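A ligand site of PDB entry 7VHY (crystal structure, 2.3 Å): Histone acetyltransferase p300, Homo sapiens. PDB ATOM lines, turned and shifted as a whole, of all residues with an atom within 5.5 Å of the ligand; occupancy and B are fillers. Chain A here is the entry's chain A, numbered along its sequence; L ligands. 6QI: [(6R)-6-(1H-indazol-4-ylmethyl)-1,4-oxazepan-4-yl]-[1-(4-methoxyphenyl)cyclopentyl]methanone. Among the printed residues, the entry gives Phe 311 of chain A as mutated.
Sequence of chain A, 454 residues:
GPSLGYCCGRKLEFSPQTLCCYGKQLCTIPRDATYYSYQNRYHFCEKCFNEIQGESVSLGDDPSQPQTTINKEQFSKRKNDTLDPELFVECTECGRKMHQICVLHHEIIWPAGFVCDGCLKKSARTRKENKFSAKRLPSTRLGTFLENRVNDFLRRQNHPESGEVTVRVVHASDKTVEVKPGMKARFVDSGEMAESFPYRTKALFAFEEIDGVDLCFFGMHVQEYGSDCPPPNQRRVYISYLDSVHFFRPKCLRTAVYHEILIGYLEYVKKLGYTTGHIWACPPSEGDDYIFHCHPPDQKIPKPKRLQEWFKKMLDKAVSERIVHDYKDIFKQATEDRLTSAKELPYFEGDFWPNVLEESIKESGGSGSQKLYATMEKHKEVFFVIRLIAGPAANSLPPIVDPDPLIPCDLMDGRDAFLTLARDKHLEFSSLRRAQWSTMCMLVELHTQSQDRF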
ATOM      1  N   PHE A 218     -30.455 -16.301 -18.212  1.00  0.00           N
ATOM      2  CA  PHE A 218     -29.057 -16.209 -18.624  1.00  0.00           C
ATOM      3  C   PHE A 218     -28.956 -15.349 -19.868  1.00  0.00           C
ATOM      4  O   PHE A 218     -29.818 -15.412 -20.753  1.00  0.00           O
ATOM      5  CB  PHE A 218     -28.465 -17.598 -18.885  1.00  0.00           C
ATOM      6  CG  PHE A 218     -27.046 -17.564 -19.378  1.00  0.00           C
ATOM      7  CD1 PHE A 218     -25.993 -17.473 -18.480  1.00  0.00           C
ATOM      8  CD2 PHE A 218     -26.765 -17.617 -20.733  1.00  0.00           C
ATOM      9  CE1 PHE A 218     -24.687 -17.442 -18.928  1.00  0.00           C
ATOM     10  CE2 PHE A 218     -25.467 -17.588 -21.186  1.00  0.00           C
ATOM     11  CZ  PHE A 218     -24.426 -17.505 -20.285  1.00  0.00           C
ATOM     12  N   LEU A 242     -21.569 -11.224 -19.186  1.00  0.00           N
ATOM     13  CA  LEU A 242     -22.416 -12.326 -18.739  1.00  0.00           C
ATOM     14  C   LEU A 242     -23.353 -11.820 -17.657  1.00  0.00           C
ATOM     15  O   LEU A 242     -23.010 -10.916 -16.885  1.00  0.00           O
ATOM     16  CB  LEU A 242     -21.587 -13.493 -18.179  1.00  0.00           C
ATOM     17  CG  LEU A 242     -20.767 -14.373 -19.125  1.00  0.00           C
ATOM     18  CD1 LEU A 242     -19.875 -15.299 -18.323  1.00  0.00           C
ATOM     19  CD2 LEU A 242     -21.686 -15.162 -20.038  1.00  0.00           C
ATOM     20  N   ASP A 243     -24.541 -12.415 -17.608  1.00  0.00           N
ATOM     21  CA  ASP A 243     -25.506 -12.032 -16.593  1.00  0.00           C
ATOM     22  C   ASP A 243     -26.472 -13.189 -16.398  1.00  0.00           C
ATOM     23  O   ASP A 243     -26.590 -14.078 -17.247  1.00  0.00           O
ATOM     24  CB  ASP A 243     -26.262 -10.753 -16.975  1.00  0.00           C
ATOM     25  CG  ASP A 243     -26.637  -9.923 -15.752  1.00  0.00           C
ATOM     26  OD1 ASP A 243     -26.499 -10.446 -14.623  1.00  0.00           O
ATOM     27  OD2 ASP A 243     -27.053  -8.763 -15.928  1.00  0.00           O
ATOM     28  N   SER A 244     -27.151 -13.163 -15.256  1.00  0.00           N
ATOM     29  CA  SER A 244     -28.064 -14.244 -14.912  1.00  0.00           C
ATOM     30  C   SER A 244     -29.113 -13.715 -13.939  1.00  0.00           C
ATOM     31  O   SER A 244     -28.900 -12.716 -13.245  1.00  0.00           O
ATOM     32  CB  SER A 244     -27.322 -15.438 -14.295  1.00  0.00           C
ATOM     33  OG  SER A 244     -26.666 -15.053 -13.094  1.00  0.00           O
ATOM     34  N   TYR A 258     -25.182 -23.374 -16.030  1.00  0.00           N
ATOM     35  CA  TYR A 258     -24.270 -22.334 -16.507  1.00  0.00           C
ATOM     36  C   TYR A 258     -23.022 -22.950 -17.122  1.00  0.00           C
ATOM     37  O   TYR A 258     -22.519 -22.484 -18.149  1.00  0.00           O
ATOM     38  CB  TYR A 258     -23.873 -21.386 -15.371  1.00  0.00           C
ATOM     39  CG  TYR A 258     -25.018 -20.590 -14.783  1.00  0.00           C
ATOM     40  CD1 TYR A 258     -26.154 -20.300 -15.536  1.00  0.00           C
ATOM     41  CD2 TYR A 258     -24.953 -20.113 -13.486  1.00  0.00           C
ATOM     42  CE1 TYR A 258     -27.191 -19.562 -14.993  1.00  0.00           C
ATOM     43  CE2 TYR A 258     -25.982 -19.372 -12.938  1.00  0.00           C
ATOM     44  CZ  TYR A 258     -27.104 -19.108 -13.699  1.00  0.00           C
ATOM     45  OH  TYR A 258     -28.133 -18.367 -13.151  1.00  0.00           O
ATOM     46  N   LEU A 262     -21.750 -22.416 -20.991  1.00  0.00           N
ATOM     47  CA  LEU A 262     -20.447 -21.804 -21.236  1.00  0.00           C
ATOM     48  C   LEU A 262     -19.492 -22.764 -21.922  1.00  0.00           C
ATOM     49  O   LEU A 262     -18.805 -22.407 -22.890  1.00  0.00           O
ATOM     50  CB  LEU A 262     -19.855 -21.303 -19.915  1.00  0.00           C
ATOM     51  CG  LEU A 262     -20.533 -20.079 -19.306  1.00  0.00           C
ATOM     52  CD1 LEU A 262     -19.714 -19.541 -18.134  1.00  0.00           C
ATOM     53  CD2 LEU A 262     -20.754 -18.993 -20.350  1.00  0.00           C
ATOM     54  N   CYS A 282     -14.573 -10.326 -14.099  1.00  0.00           N
ATOM     55  CA  CYS A 282     -14.802  -9.017 -13.491  1.00  0.00           C
ATOM     56  C   CYS A 282     -16.227  -8.933 -12.973  1.00  0.00           C
ATOM     57  O   CYS A 282     -17.172  -8.777 -13.764  1.00  0.00           O
ATOM     58  CB  CYS A 282     -14.524  -7.905 -14.486  1.00  0.00           C
ATOM     59  SG  CYS A 282     -14.591  -6.235 -13.783  1.00  0.00           S
ATOM     60  N   PRO A 283     -16.431  -9.038 -11.657  1.00  0.00           N
ATOM     61  CA  PRO A 283     -17.778  -8.876 -11.110  1.00  0.00           C
ATOM     62  C   PRO A 283     -18.242  -7.432 -11.263  1.00  0.00           C
ATOM     63  O   PRO A 283     -17.421  -6.494 -11.262  1.00  0.00           O
ATOM     64  CB  PRO A 283     -17.613  -9.247  -9.632  1.00  0.00           C
ATOM     65  CG  PRO A 283     -16.192  -8.977  -9.328  1.00  0.00           C
ATOM     66  CD  PRO A 283     -15.424  -9.208 -10.603  1.00  0.00           C
ATOM     67  N   PRO A 284     -19.545  -7.204 -11.417  1.00  0.00           N
ATOM     68  CA  PRO A 284     -20.029  -5.834 -11.557  1.00  0.00           C
ATOM     69  C   PRO A 284     -19.935  -5.077 -10.243  1.00  0.00           C
ATOM     70  O   PRO A 284     -19.945  -5.667  -9.153  1.00  0.00           O
ATOM     71  CB  PRO A 284     -21.488  -6.014 -11.987  1.00  0.00           C
ATOM     72  CG  PRO A 284     -21.869  -7.353 -11.453  1.00  0.00           C
ATOM     73  CD  PRO A 284     -20.624  -8.198 -11.524  1.00  0.00           C
ATOM     74  N   ASP A 288     -24.671  -1.932 -10.149  1.00  0.00           N
ATOM     75  CA  ASP A 288     -24.466  -1.985 -11.598  1.00  0.00           C
ATOM     76  C   ASP A 288     -25.128  -3.225 -12.167  1.00  0.00           C
ATOM     77  O   ASP A 288     -25.113  -4.300 -11.548  1.00  0.00           O
ATOM     78  CB  ASP A 288     -22.975  -1.985 -11.933  1.00  0.00           C
ATOM     79  CG  ASP A 288     -22.608  -0.961 -12.985  1.00  0.00           C
ATOM     80  OD1 ASP A 288     -23.341  -0.846 -13.998  1.00  0.00           O
ATOM     81  OD2 ASP A 288     -21.592  -0.247 -12.801  1.00  0.00           O
ATOM     82  N   ASP A 289     -25.728  -3.082 -13.351  1.00  0.00           N
ATOM     83  CA  ASP A 289     -26.369  -4.189 -14.046  1.00  0.00           C
ATOM     84  C   ASP A 289     -25.651  -4.418 -15.378  1.00  0.00           C
ATOM     85  O   ASP A 289     -25.500  -3.483 -16.171  1.00  0.00           O
ATOM     86  CB  ASP A 289     -27.854  -3.887 -14.300  1.00  0.00           C
ATOM     87  CG  ASP A 289     -28.665  -3.846 -13.012  1.00  0.00           C
ATOM     88  OD1 ASP A 289     -28.406  -4.668 -12.114  1.00  0.00           O
ATOM     89  OD2 ASP A 289     -29.559  -2.978 -12.909  1.00  0.00           O
ATOM     90  N   TYR A 290     -25.227  -5.658 -15.608  1.00  0.00           N
ATOM     91  CA  TYR A 290     -24.550  -5.980 -16.862  1.00  0.00           C
ATOM     92  C   TYR A 290     -25.534  -6.059 -18.017  1.00  0.00           C
ATOM     93  O   TYR A 290     -25.456  -5.287 -18.978  1.00  0.00           O
ATOM     94  CB  TYR A 290     -23.783  -7.297 -16.715  1.00  0.00           C
ATOM     95  CG  TYR A 290     -22.379  -7.144 -16.141  1.00  0.00           C
ATOM     96  CD1 TYR A 290     -21.823  -5.892 -15.940  1.00  0.00           C
ATOM     97  CD2 TYR A 290     -21.625  -8.257 -15.805  1.00  0.00           C
ATOM     98  CE1 TYR A 290     -20.556  -5.748 -15.419  1.00  0.00           C
ATOM     99  CE2 TYR A 290     -20.352  -8.134 -15.280  1.00  0.00           C
ATOM    100  CZ  TYR A 290     -19.818  -6.880 -15.087  1.00  0.00           C
ATOM    101  OH  TYR A 290     -18.546  -6.744 -14.568  1.00  0.00           O
ATOM    102  N   ILE A 291     -26.484  -7.005 -17.944  1.00  0.00           N
ATOM    103  CA  ILE A 291     -27.465  -7.210 -18.995  1.00  0.00           C
ATOM    104  C   ILE A 291     -28.889  -7.069 -18.469  1.00  0.00           C
ATOM    105  O   ILE A 291     -29.739  -6.444 -19.136  1.00  0.00           O
ATOM    106  CB  ILE A 291     -27.271  -8.588 -19.667  1.00  0.00           C
ATOM    107  CG1 ILE A 291     -25.881  -8.690 -20.296  1.00  0.00           C
ATOM    108  CG2 ILE A 291     -28.348  -8.830 -20.719  1.00  0.00           C
ATOM    109  CD1 ILE A 291     -25.550 -10.081 -20.806  1.00  0.00           C
ATOM    110  N   PHE A 292     -29.189  -7.644 -17.315  1.00  0.00           N
ATOM    111  CA  PHE A 292     -30.529  -7.669 -16.757  1.00  0.00           C
ATOM    112  C   PHE A 292     -30.699  -6.533 -15.755  1.00  0.00           C
ATOM    113  O   PHE A 292     -29.886  -6.389 -14.835  1.00  0.00           O
ATOM    114  CB  PHE A 292     -30.833  -9.015 -16.107  1.00  0.00           C
ATOM    115  CG  PHE A 292     -30.828 -10.168 -17.070  1.00  0.00           C
ATOM    116  CD1 PHE A 292     -31.798 -10.255 -18.064  1.00  0.00           C
ATOM    117  CD2 PHE A 292     -29.861 -11.154 -17.009  1.00  0.00           C
ATOM    118  CE1 PHE A 292     -31.796 -11.316 -18.953  1.00  0.00           C
ATOM    119  CE2 PHE A 292     -29.859 -12.214 -17.898  1.00  0.00           C
ATOM    120  CZ  PHE A 292     -30.829 -12.294 -18.877  1.00  0.00           C
ATOM    121  N   HIS A 295     -31.506  -6.688 -10.650  1.00  0.00           N
ATOM    122  CA  HIS A 295     -31.310  -8.027 -10.119  1.00  0.00           C
ATOM    123  C   HIS A 295     -32.009  -8.182  -8.767  1.00  0.00           C
ATOM    124  O   HIS A 295     -32.303  -7.197  -8.095  1.00  0.00           O
ATOM    125  CB  HIS A 295     -29.811  -8.319  -9.952  1.00  0.00           C
ATOM    126  CG  HIS A 295     -29.100  -8.563 -11.246  1.00  0.00           C
ATOM    127  ND1 HIS A 295     -28.693  -7.530 -12.069  1.00  0.00           N
ATOM    128  CD2 HIS A 295     -28.720  -9.712 -11.848  1.00  0.00           C
ATOM    129  CE1 HIS A 295     -28.094  -8.045 -13.133  1.00  0.00           C
ATOM    130  NE2 HIS A 295     -28.089  -9.355 -13.023  1.00  0.00           N
ATOM    131  N   GLN A 299     -29.490 -11.744  -4.673  1.00  0.00           N
ATOM    132  CA  GLN A 299     -28.535 -12.343  -5.614  1.00  0.00           C
ATOM    133  C   GLN A 299     -27.224 -11.582  -5.459  1.00  0.00           C
ATOM    134  O   GLN A 299     -27.033 -10.518  -6.030  1.00  0.00           O
ATOM    135  CB  GLN A 299     -29.064 -12.285  -7.044  1.00  0.00           C
ATOM    136  CG  GLN A 299     -28.184 -13.036  -8.040  1.00  0.00           C
ATOM    137  CD  GLN A 299     -28.717 -12.982  -9.461  1.00  0.00           C
ATOM    138  OE1 GLN A 299     -29.916 -12.868  -9.680  1.00  0.00           O
ATOM    139  NE2 GLN A 299     -27.816 -13.074 -10.432  1.00  0.00           N
ATOM    140  N   LYS A 300     -26.317 -12.154  -4.677  1.00  0.00           N
ATOM    141  CA  LYS A 300     -25.084 -11.469  -4.293  1.00  0.00           C
ATOM    142  C   LYS A 300     -24.067 -11.474  -5.422  1.00  0.00           C
ATOM    143  O   LYS A 300     -23.970 -12.435  -6.203  1.00  0.00           O
ATOM    144  CB  LYS A 300     -24.490 -12.117  -3.044  1.00  0.00           C
ATOM    145  CG  LYS A 300     -25.326 -11.925  -1.796  1.00  0.00           C
ATOM    146  CD  LYS A 300     -25.506 -13.230  -1.033  1.00  0.00           C
ATOM    147  CE  LYS A 300     -24.450 -13.383   0.052  1.00  0.00           C
ATOM    148  NZ  LYS A 300     -24.785 -12.603   1.277  1.00  0.00           N
ATOM    149  N   ILE A 301     -23.310 -10.388  -5.515  1.00  0.00           N
ATOM    150  CA  ILE A 301     -22.199 -10.276  -6.443  1.00  0.00           C
ATOM    151  C   ILE A 301     -20.983 -10.971  -5.837  1.00  0.00           C
ATOM    152  O   ILE A 301     -20.580 -10.637  -4.713  1.00  0.00           O
ATOM    153  CB  ILE A 301     -21.877  -8.807  -6.775  1.00  0.00           C
ATOM    154  CG1 ILE A 301     -23.169  -8.007  -6.980  1.00  0.00           C
ATOM    155  CG2 ILE A 301     -20.970  -8.705  -7.980  1.00  0.00           C
ATOM    156  CD1 ILE A 301     -22.946  -6.509  -7.047  1.00  0.00           C
ATOM    157  N   PRO A 302     -20.403 -11.955  -6.517  1.00  0.00           N
ATOM    158  CA  PRO A 302     -19.225 -12.633  -5.955  1.00  0.00           C
ATOM    159  C   PRO A 302     -18.029 -11.700  -5.866  1.00  0.00           C
ATOM    160  O   PRO A 302     -17.865 -10.777  -6.672  1.00  0.00           O
ATOM    161  CB  PRO A 302     -18.968 -13.776  -6.936  1.00  0.00           C
ATOM    162  CG  PRO A 302     -19.558 -13.303  -8.216  1.00  0.00           C
ATOM    163  CD  PRO A 302     -20.749 -12.462  -7.856  1.00  0.00           C
ATOM    164  N   ARG A 306     -13.420 -15.215  -5.473  1.00  0.00           N
ATOM    165  CA  ARG A 306     -14.416 -16.262  -5.646  1.00  0.00           C
ATOM    166  C   ARG A 306     -14.759 -16.470  -7.114  1.00  0.00           C
ATOM    167  O   ARG A 306     -14.855 -17.605  -7.587  1.00  0.00           O
ATOM    168  CB  ARG A 306     -15.671 -15.930  -4.846  1.00  0.00           C
ATOM    169  CG  ARG A 306     -16.885 -16.768  -5.196  1.00  0.00           C
ATOM    170  CD  ARG A 306     -17.879 -16.806  -4.043  1.00  0.00           C
ATOM    171  NE  ARG A 306     -18.884 -17.849  -4.242  1.00  0.00           N
ATOM    172  CZ  ARG A 306     -20.175 -17.615  -4.399  1.00  0.00           C
ATOM    173  NH1 ARG A 306     -20.671 -16.386  -4.365  1.00  0.00           N
ATOM    174  NH2 ARG A 306     -20.998 -18.635  -4.591  1.00  0.00           N
ATOM    175  N   LEU A 307     -14.947 -15.377  -7.859  1.00  0.00           N
ATOM    176  CA  LEU A 307     -15.287 -15.482  -9.270  1.00  0.00           C
ATOM    177  C   LEU A 307     -14.175 -16.161 -10.065  1.00  0.00           C
ATOM    178  O   LEU A 307     -14.453 -16.984 -10.948  1.00  0.00           O
ATOM    179  CB  LEU A 307     -15.589 -14.102  -9.849  1.00  0.00           C
ATOM    180  CG  LEU A 307     -16.107 -14.094 -11.289  1.00  0.00           C
ATOM    181  CD1 LEU A 307     -17.346 -14.964 -11.424  1.00  0.00           C
ATOM    182  CD2 LEU A 307     -16.388 -12.669 -11.749  1.00  0.00           C
ATOM    183  N   TRP A 310     -14.320 -19.804  -9.491  1.00  0.00           N
ATOM    184  CA  TRP A 310     -15.478 -20.367 -10.179  1.00  0.00           C
ATOM    185  C   TRP A 310     -15.166 -20.654 -11.635  1.00  0.00           C
ATOM    186  O   TRP A 310     -15.518 -21.718 -12.169  1.00  0.00           O
ATOM    187  CB  TRP A 310     -16.662 -19.415 -10.048  1.00  0.00           C
ATOM    188  CG  TRP A 310     -17.960 -19.959 -10.580  1.00  0.00           C
ATOM    189  CD1 TRP A 310     -18.936 -20.611  -9.873  1.00  0.00           C
ATOM    190  CD2 TRP A 310     -18.457 -19.863 -11.926  1.00  0.00           C
ATOM    191  NE1 TRP A 310     -19.981 -20.944 -10.692  1.00  0.00           N
ATOM    192  CE2 TRP A 310     -19.710 -20.500 -11.965  1.00  0.00           C
ATOM    193  CE3 TRP A 310     -17.935 -19.315 -13.107  1.00  0.00           C
ATOM    194  CZ2 TRP A 310     -20.468 -20.589 -13.124  1.00  0.00           C
ATOM    195  CZ3 TRP A 310     -18.689 -19.412 -14.268  1.00  0.00           C
ATOM    196  CH2 TRP A 310     -19.940 -20.049 -14.270  1.00  0.00           C
ATOM    197  N   PHE A 311     -14.496 -19.713 -12.320  1.00  0.00           N
ATOM    198  CA  PHE A 311     -14.109 -19.924 -13.702  1.00  0.00           C
ATOM    199  C   PHE A 311     -13.102 -21.055 -13.824  1.00  0.00           C
ATOM    200  O   PHE A 311     -13.132 -21.823 -14.801  1.00  0.00           O
ATOM    201  CB  PHE A 311     -13.559 -18.639 -14.301  1.00  0.00           C
ATOM    202  CG  PHE A 311     -14.627 -17.698 -14.807  1.00  0.00           C
ATOM    203  CD1 PHE A 311     -15.420 -18.054 -15.881  1.00  0.00           C
ATOM    204  CD2 PHE A 311     -14.831 -16.470 -14.196  1.00  0.00           C
ATOM    205  CE1 PHE A 311     -16.404 -17.201 -16.337  1.00  0.00           C
ATOM    206  CE2 PHE A 311     -15.802 -15.610 -14.655  1.00  0.00           C
ATOM    207  CZ  PHE A 311     -16.599 -15.970 -15.721  1.00  0.00           C
HETATM  208  CAA 6QI L   1     -22.339 -15.843  -9.793  1.00  0.00           C
HETATM  209  CAB 6QI L   1     -22.747 -15.621 -11.093  1.00  0.00           C
HETATM  210  CAC 6QI L   1     -22.002 -16.107 -12.151  1.00  0.00           C
HETATM  211  CAD 6QI L   1     -20.845 -16.825 -11.912  1.00  0.00           C
HETATM  212  CAE 6QI L   1     -20.440 -17.052 -10.603  1.00  0.00           C
HETATM  213  CAF 6QI L   1     -21.190 -16.557  -9.543  1.00  0.00           C
HETATM  214  CAH 6QI L   1     -19.501 -17.345  -8.245  1.00  0.00           C
HETATM  215  CAI 6QI L   1     -22.417 -15.850 -13.460  1.00  0.00           C
HETATM  216  CAJ 6QI L   1     -22.853 -14.351 -13.668  1.00  0.00           C
HETATM  217  CAL 6QI L   1     -22.662 -11.990 -13.660  1.00  0.00           C
HETATM  218  CAM 6QI L   1     -22.920 -11.293 -12.337  1.00  0.00           C
HETATM  219  CAN 6QI L   1     -22.149 -11.964 -11.242  1.00  0.00           C
HETATM  220  CAP 6QI L   1     -20.188 -11.957 -12.537  1.00  0.00           C
HETATM  221  CAQ 6QI L   1     -20.598 -13.316 -13.013  1.00  0.00           C
HETATM  222  CAR 6QI L   1     -24.416 -11.369 -12.032  1.00  0.00           C
HETATM  223  CAS 6QI L   1     -24.872 -10.300 -11.264  1.00  0.00           C
HETATM  224  CAT 6QI L   1     -24.971  -9.068 -11.774  1.00  0.00           C
HETATM  225  CAU 6QI L   1     -25.408  -8.060 -11.042  1.00  0.00           C
HETATM  226  CAV 6QI L   1     -25.769  -8.221  -9.777  1.00  0.00           C
HETATM  227  CAW 6QI L   1     -25.700  -9.468  -9.191  1.00  0.00           C
HETATM  228  CAX 6QI L   1     -25.245 -10.517  -9.949  1.00  0.00           C
HETATM  229  CBA 6QI L   1     -24.719  -8.523 -12.952  1.00  0.00           C
HETATM  230  CBC 6QI L   1     -23.607 -16.709 -13.737  1.00  0.00           C
HETATM  231  CBD 6QI L   1     -23.512 -17.188 -15.172  1.00  0.00           C
HETATM  232  CBE 6QI L   1     -22.253 -16.604 -15.707  1.00  0.00           C
HETATM  233  CBF 6QI L   1     -21.428 -16.359 -14.484  1.00  0.00           C
HETATM  234  NAK 6QI L   1     -22.016 -13.286 -13.445  1.00  0.00           N
HETATM  235  NAY 6QI L   1     -25.382  -7.003 -11.836  1.00  0.00           N
HETATM  236  NAZ 6QI L   1     -25.015  -7.244 -12.853  1.00  0.00           N
HETATM  237  OAG 6QI L   1     -20.803 -16.770  -8.272  1.00  0.00           O
HETATM  238  OAO 6QI L   1     -20.781 -11.649 -11.290  1.00  0.00           O
HETATM  239  OBB 6QI L   1     -24.013 -14.145 -14.002  1.00  0.00           O
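A nitrogen (NAY) of the ligand sits at hydrogen-bond distance from the backbone carbonyl oxygen (O) of Asp 288, 2.7 Å away. OG of Ser 244 sits at hydrogen-bond distance from OBB of the ligand, 2.9 Å away. A nitrogen (NAY) of the ligand lies close to a ring nitrogen (ND1) of His 295. A nitrogen (NAZ) of the ligand is in hydrogen-bond range of the backbone NH of Tyr 290 (3.2 Å).
O of Ser 244 sits close to NE2 of His 295. The backbone carbonyl oxygen (O) of Ser 244 lies within hydrogen-bond range of the side-chain amide nitrogen (NE2) of Gln 299, at 3.0 Å. OD1 of Asp 243 is in hydrogen-bond range of NE2 of His 295, at 2.5 Å. The side-chain carboxylate (OD2) of Asp 243 is in hydrogen-bond range of the backbone NH (N) of Ile 291 (2.7 Å). OD2 of Asp 243 sits at hydrogen-bond distance from N of Phe 292 (2.8 Å). OD1 of Asp 289 sits at hydrogen-bond distance from ND1 of His 295 (2.9 Å). The backbone carbonyl oxygen (O) of Phe 292 sits close to a ring nitrogen (ND1) of His 295 (3.2 Å). The side-chain hydroxyl of Tyr 290 is in hydrogen-bond range of the backbone carbonyl oxygen of Cys 282 (2.6 Å).
Phe 218 touches the ligand. Leu 242 touches the ligand. Asp 243 touches the ligand. CE2 of Tyr 258 touches CBC of the ligand, at 3.7 Å. CG of Pro 284 touches CBA of the ligand (3.4 Å). CA of Asp 289 touches NAZ of the ligand, 3.5 Å away. Gln 299 touches the ligand. CG1 of Ile 301 touches CAW of the ligand, 3.7 Å away. Pro 302 touches the ligand. Arg 306 touches the ligand (CZ to CAH, 3.9 Å). CD1 of Leu 307 touches CAE of the ligand (3.8 Å). Trp 310 touches the ligand (CD2 to CAE, 3.7 Å). Hydrophobic or aromatic side chains that line the ligand: Phe 218, Leu 242, Tyr 258, Pro 284, His 295, Ile 301, Pro 302, Leu 307 and Trp 310. 16 residues have an atom within 4 Å of the ligand: Phe 218, Leu 242, Asp 243, Ser 244, Tyr 258, Pro 284, Asp 288, Asp 289, Tyr 290, His 295, Gln 299, Ile 301, Pro 302, Arg 306, Leu 307 and Trp 310. Along chain A the residues within 4 Å of the ligand span positions 218 to 310. The nearest printed residue that does not touch the ligand is Pro 283 (4.1 Å).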
